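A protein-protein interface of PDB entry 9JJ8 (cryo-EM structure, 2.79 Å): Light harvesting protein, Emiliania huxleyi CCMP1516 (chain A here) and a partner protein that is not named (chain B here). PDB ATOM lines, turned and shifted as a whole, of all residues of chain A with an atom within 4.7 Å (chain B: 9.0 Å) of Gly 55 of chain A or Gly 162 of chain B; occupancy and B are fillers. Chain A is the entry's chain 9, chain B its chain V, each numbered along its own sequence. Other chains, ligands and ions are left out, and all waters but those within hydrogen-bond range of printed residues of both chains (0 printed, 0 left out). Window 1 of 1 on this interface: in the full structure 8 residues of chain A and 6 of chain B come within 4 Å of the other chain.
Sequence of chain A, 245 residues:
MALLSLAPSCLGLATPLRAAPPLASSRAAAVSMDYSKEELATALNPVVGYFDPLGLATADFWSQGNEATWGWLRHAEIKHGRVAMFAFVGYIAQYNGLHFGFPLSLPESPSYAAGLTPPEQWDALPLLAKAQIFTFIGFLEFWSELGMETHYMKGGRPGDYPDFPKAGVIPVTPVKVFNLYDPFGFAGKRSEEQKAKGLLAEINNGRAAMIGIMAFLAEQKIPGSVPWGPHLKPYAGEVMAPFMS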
ATOM      1  N   ASP A  52      28.360  32.265 -18.842  1.00  0.00           N
ATOM      2  CA  ASP A  52      28.068  30.896 -19.260  1.00  0.00           C
ATOM      3  C   ASP A  52      28.896  30.557 -20.499  1.00  0.00           C
ATOM      4  O   ASP A  52      28.530  30.929 -21.624  1.00  0.00           O
ATOM      5  CB  ASP A  52      26.564  30.659 -19.487  1.00  0.00           C
ATOM      6  CG  ASP A  52      25.885  31.701 -20.398  1.00  0.00           C
ATOM      7  OD1 ASP A  52      26.527  32.697 -20.795  1.00  0.00           O
ATOM      8  OD2 ASP A  52      24.682  31.505 -20.708  1.00  0.00           O
ATOM      9  N   PRO A  53      30.041  29.878 -20.343  1.00  0.00           N
ATOM     10  CA  PRO A  53      30.670  29.263 -21.522  1.00  0.00           C
ATOM     11  C   PRO A  53      29.776  28.253 -22.211  1.00  0.00           C
ATOM     12  O   PRO A  53      29.882  28.089 -23.432  1.00  0.00           O
ATOM     13  CB  PRO A  53      31.940  28.609 -20.957  1.00  0.00           C
ATOM     14  CG  PRO A  53      32.187  29.300 -19.701  1.00  0.00           C
ATOM     15  CD  PRO A  53      30.851  29.657 -19.134  1.00  0.00           C
ATOM     16  N   LEU A  54      28.904  27.574 -21.469  1.00  0.00           N
ATOM     17  CA  LEU A  54      27.848  26.743 -22.037  1.00  0.00           C
ATOM     18  C   LEU A  54      26.519  27.476 -21.908  1.00  0.00           C
ATOM     19  O   LEU A  54      26.083  27.775 -20.793  1.00  0.00           O
ATOM     20  CB  LEU A  54      27.766  25.393 -21.327  1.00  0.00           C
ATOM     21  CG  LEU A  54      28.582  24.217 -21.862  1.00  0.00           C
ATOM     22  CD1 LEU A  54      30.073  24.472 -21.767  1.00  0.00           C
ATOM     23  CD2 LEU A  54      28.208  22.959 -21.095  1.00  0.00           C
ATOM     24  N   GLY A  55      25.856  27.722 -23.037  1.00  0.00           N
ATOM     25  CA  GLY A  55      24.610  28.468 -23.029  1.00  0.00           C
ATOM     26  C   GLY A  55      23.395  27.715 -22.516  1.00  0.00           C
ATOM     27  O   GLY A  55      22.399  27.571 -23.230  1.00  0.00           O
ATOM     28  N   LEU A  56      23.459  27.244 -21.266  1.00  0.00           N
ATOM     29  CA  LEU A  56      22.369  26.447 -20.710  1.00  0.00           C
ATOM     30  C   LEU A  56      21.187  27.309 -20.286  1.00  0.00           C
ATOM     31  O   LEU A  56      20.047  26.835 -20.282  1.00  0.00           O
ATOM     32  CB  LEU A  56      22.887  25.612 -19.543  1.00  0.00           C
ATOM     33  CG  LEU A  56      23.892  24.557 -20.006  1.00  0.00           C
ATOM     34  CD1 LEU A  56      24.510  23.849 -18.833  1.00  0.00           C
ATOM     35  CD2 LEU A  56      23.217  23.553 -20.924  1.00  0.00           C
ATOM     36  N   ALA A  57      21.434  28.560 -19.907  1.00  0.00           N
ATOM     37  CA  ALA A  57      20.342  29.512 -19.799  1.00  0.00           C
ATOM     38  C   ALA A  57      19.838  29.865 -21.195  1.00  0.00           C
ATOM     39  O   ALA A  57      20.586  29.828 -22.178  1.00  0.00           O
ATOM     40  CB  ALA A  57      20.788  30.768 -19.053  1.00  0.00           C
ATOM     41  N   ALA A  59      17.921  27.975 -22.841  1.00  0.00           N
ATOM     42  CA  ALA A  59      17.793  26.729 -23.581  1.00  0.00           C
ATOM     43  C   ALA A  59      16.321  26.327 -23.615  1.00  0.00           C
ATOM     44  O   ALA A  59      15.433  27.115 -23.278  1.00  0.00           O
ATOM     45  CB  ALA A  59      18.668  25.643 -22.961  1.00  0.00           C
ATOM     46  N   LEU B 156      12.756  16.992 -31.931  1.00  0.00           N
ATOM     47  CA  LEU B 156      13.472  17.487 -30.756  1.00  0.00           C
ATOM     48  C   LEU B 156      14.948  17.078 -30.774  1.00  0.00           C
ATOM     49  O   LEU B 156      15.785  17.763 -30.175  1.00  0.00           O
ATOM     50  CB  LEU B 156      12.795  17.022 -29.456  1.00  0.00           C
ATOM     51  CG  LEU B 156      13.402  17.640 -28.183  1.00  0.00           C
ATOM     52  CD1 LEU B 156      13.211  19.151 -28.205  1.00  0.00           C
ATOM     53  CD2 LEU B 156      12.882  17.075 -26.893  1.00  0.00           C
ATOM     54  N   TRP B 158      17.756  17.112 -32.198  1.00  0.00           N
ATOM     55  CA  TRP B 158      18.897  18.008 -32.288  1.00  0.00           C
ATOM     56  C   TRP B 158      18.832  19.070 -31.201  1.00  0.00           C
ATOM     57  O   TRP B 158      17.780  19.672 -30.963  1.00  0.00           O
ATOM     58  CB  TRP B 158      18.956  18.680 -33.658  1.00  0.00           C
ATOM     59  CG  TRP B 158      19.872  19.855 -33.697  1.00  0.00           C
ATOM     60  CD1 TRP B 158      19.526  21.156 -33.902  1.00  0.00           C
ATOM     61  CD2 TRP B 158      21.293  19.838 -33.534  1.00  0.00           C
ATOM     62  NE1 TRP B 158      20.643  21.954 -33.871  1.00  0.00           N
ATOM     63  CE2 TRP B 158      21.742  21.167 -33.648  1.00  0.00           C
ATOM     64  CE3 TRP B 158      22.230  18.828 -33.302  1.00  0.00           C
ATOM     65  CZ2 TRP B 158      23.083  21.509 -33.537  1.00  0.00           C
ATOM     66  CZ3 TRP B 158      23.558  19.170 -33.192  1.00  0.00           C
ATOM     67  CH2 TRP B 158      23.973  20.498 -33.308  1.00  0.00           C
ATOM     68  N   ASP B 159      19.976  19.294 -30.548  1.00  0.00           N
ATOM     69  CA  ASP B 159      20.189  20.287 -29.499  1.00  0.00           C
ATOM     70  C   ASP B 159      19.237  20.116 -28.321  1.00  0.00           C
ATOM     71  O   ASP B 159      18.330  20.936 -28.137  1.00  0.00           O
ATOM     72  CB  ASP B 159      20.068  21.701 -30.068  1.00  0.00           C
ATOM     73  CG  ASP B 159      20.720  22.735 -29.184  1.00  0.00           C
ATOM     74  OD1 ASP B 159      21.633  22.367 -28.417  1.00  0.00           O
ATOM     75  OD2 ASP B 159      20.317  23.913 -29.251  1.00  0.00           O
ATOM     76  N   PRO B 160      19.396  19.068 -27.505  1.00  0.00           N
ATOM     77  CA  PRO B 160      18.570  18.976 -26.294  1.00  0.00           C
ATOM     78  C   PRO B 160      19.012  19.931 -25.203  1.00  0.00           C
ATOM     79  O   PRO B 160      18.181  20.360 -24.393  1.00  0.00           O
ATOM     80  CB  PRO B 160      18.739  17.510 -25.860  1.00  0.00           C
ATOM     81  CG  PRO B 160      19.527  16.837 -26.962  1.00  0.00           C
ATOM     82  CD  PRO B 160      20.311  17.923 -27.610  1.00  0.00           C
ATOM     83  N   LEU B 161      20.297  20.282 -25.162  1.00  0.00           N
ATOM     84  CA  LEU B 161      20.864  21.107 -24.105  1.00  0.00           C
ATOM     85  C   LEU B 161      20.859  22.593 -24.435  1.00  0.00           C
ATOM     86  O   LEU B 161      21.319  23.395 -23.617  1.00  0.00           O
ATOM     87  CB  LEU B 161      22.299  20.658 -23.805  1.00  0.00           C
ATOM     88  CG  LEU B 161      22.538  19.750 -22.596  1.00  0.00           C
ATOM     89  CD1 LEU B 161      21.674  18.504 -22.659  1.00  0.00           C
ATOM     90  CD2 LEU B 161      24.008  19.374 -22.505  1.00  0.00           C
ATOM     91  N   GLY B 162      20.343  22.982 -25.595  1.00  0.00           N
ATOM     92  CA  GLY B 162      20.378  24.380 -25.989  1.00  0.00           C
ATOM     93  C   GLY B 162      21.759  24.921 -26.293  1.00  0.00           C
ATOM     94  O   GLY B 162      22.091  26.035 -25.870  1.00  0.00           O
ATOM     95  N   PHE B 163      22.580  24.152 -27.011  1.00  0.00           N
ATOM     96  CA  PHE B 163      23.874  24.635 -27.480  1.00  0.00           C
ATOM     97  C   PHE B 163      23.753  25.521 -28.714  1.00  0.00           C
ATOM     98  O   PHE B 163      24.756  26.105 -29.138  1.00  0.00           O
ATOM     99  CB  PHE B 163      24.799  23.451 -27.778  1.00  0.00           C
ATOM    100  CG  PHE B 163      25.545  22.939 -26.575  1.00  0.00           C
ATOM    101  CD1 PHE B 163      26.542  21.988 -26.720  1.00  0.00           C
ATOM    102  CD2 PHE B 163      25.252  23.407 -25.302  1.00  0.00           C
ATOM    103  CE1 PHE B 163      27.232  21.511 -25.619  1.00  0.00           C
ATOM    104  CE2 PHE B 163      25.938  22.934 -24.197  1.00  0.00           C
ATOM    105  CZ  PHE B 163      26.929  21.985 -24.358  1.00  0.00           C
ATOM    106  N   THR B 164      22.556  25.636 -29.286  1.00  0.00           N
ATOM    107  CA  THR B 164      22.281  26.545 -30.393  1.00  0.00           C
ATOM    108  C   THR B 164      21.333  27.624 -29.886  1.00  0.00           C
ATOM    109  O   THR B 164      20.319  27.939 -30.517  1.00  0.00           O
ATOM    110  CB  THR B 164      21.697  25.811 -31.600  1.00  0.00           C
ATOM    111  OG1 THR B 164      20.503  25.120 -31.217  1.00  0.00           O
ATOM    112  CG2 THR B 164      22.706  24.816 -32.149  1.00  0.00           C
ATOM    113  N   ALA B 165      21.683  28.184 -28.732  1.00  0.00           N
ATOM    114  CA  ALA B 165      20.911  29.164 -27.977  1.00  0.00           C
ATOM    115  C   ALA B 165      21.012  30.546 -28.609  1.00  0.00           C
ATOM    116  O   ALA B 165      21.260  30.669 -29.814  1.00  0.00           O
ATOM    117  CB  ALA B 165      21.377  29.210 -26.522  1.00  0.00           C
ATOM    118  N   LYS B 166      20.817  31.590 -27.798  1.00  0.00           N
ATOM    119  CA  LYS B 166      20.543  32.976 -28.187  1.00  0.00           C
ATOM    120  C   LYS B 166      21.496  33.615 -29.201  1.00  0.00           C
ATOM    121  O   LYS B 166      21.311  34.790 -29.536  1.00  0.00           O
ATOM    122  CB  LYS B 166      20.555  33.862 -26.941  1.00  0.00           C
ATOM    123  CG  LYS B 166      21.936  33.952 -26.300  1.00  0.00           C
ATOM    124  CD  LYS B 166      21.964  34.880 -25.097  1.00  0.00           C
ATOM    125  CE  LYS B 166      21.252  34.273 -23.906  1.00  0.00           C
ATOM    126  NZ  LYS B 166      21.958  33.067 -23.393  1.00  0.00           N
ATOM    127  N   LEU B 167      22.549  32.889 -29.607  1.00  0.00           N
ATOM    128  CA  LEU B 167      23.524  33.311 -30.616  1.00  0.00           C
ATOM    129  C   LEU B 167      22.874  33.992 -31.816  1.00  0.00           C
ATOM    130  O   LEU B 167      21.798  33.595 -32.274  1.00  0.00           O
ATOM    131  CB  LEU B 167      24.320  32.095 -31.105  1.00  0.00           C
ATOM    132  CG  LEU B 167      24.828  31.063 -30.095  1.00  0.00           C
ATOM    133  CD1 LEU B 167      25.613  29.973 -30.811  1.00  0.00           C
ATOM    134  CD2 LEU B 167      25.682  31.718 -29.022  1.00  0.00           C
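O of Gly 55 of chain A lies close to O of Gly 162 of chain B.
The side-chain carboxylate of Asp 159 of chain B is in hydrogen-bond range of the backbone NH of Gly 162 of chain B (3.2 Å). N of Phe 163 of chain B is in hydrogen-bond range of OD1 of Asp 159 of chain B (2.5 Å).
CZ of Phe 163 of chain B touches CD2 of Leu 54 of chain A, 3.6 Å away. Gly 55 of chain A touches Ala 165 of chain B (O to CB, 3.8 Å). Leu 56 of chain A touches Leu 161 of chain B (CD2 to O, 3.3 Å). O of Ala 57 of chain A touches NZ of Lys 166 of chain B, at 3.7 Å. Ala 59 of chain A touches Leu 161 of chain B. Ala 59 of chain A touches Gly 162 of chain B (CB to CA, 3.7 Å).
Gly 55 of chain A touches two residues of chain B. Printed residues of chain B within 4 Å of Ala 59 of chain A: Leu 161 and Gly 162. Of chain A, only Gly 55 (3.1 Å) and Ala 59 (3.7 Å) come within 4 Å of Gly 162 of chain B. Of the printed residues of chain A, Lys 166 of chain B touches Ala 57. The nearest printed residue of chain A that does not touch Gly 162 of chain B is Leu 56 of chain A (5.0 Å).
Printed residues of chain B that touch a printed residue of chain A: Leu 161, Gly 162, Phe 163, Ala 165 and Lys 166. Among the printed residues, 7 pairs touch across the chains. Among the printed residues, no Asp or Glu carboxylate lies within 4 Å of a Lys or Arg side-chain nitrogen of the other chain.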
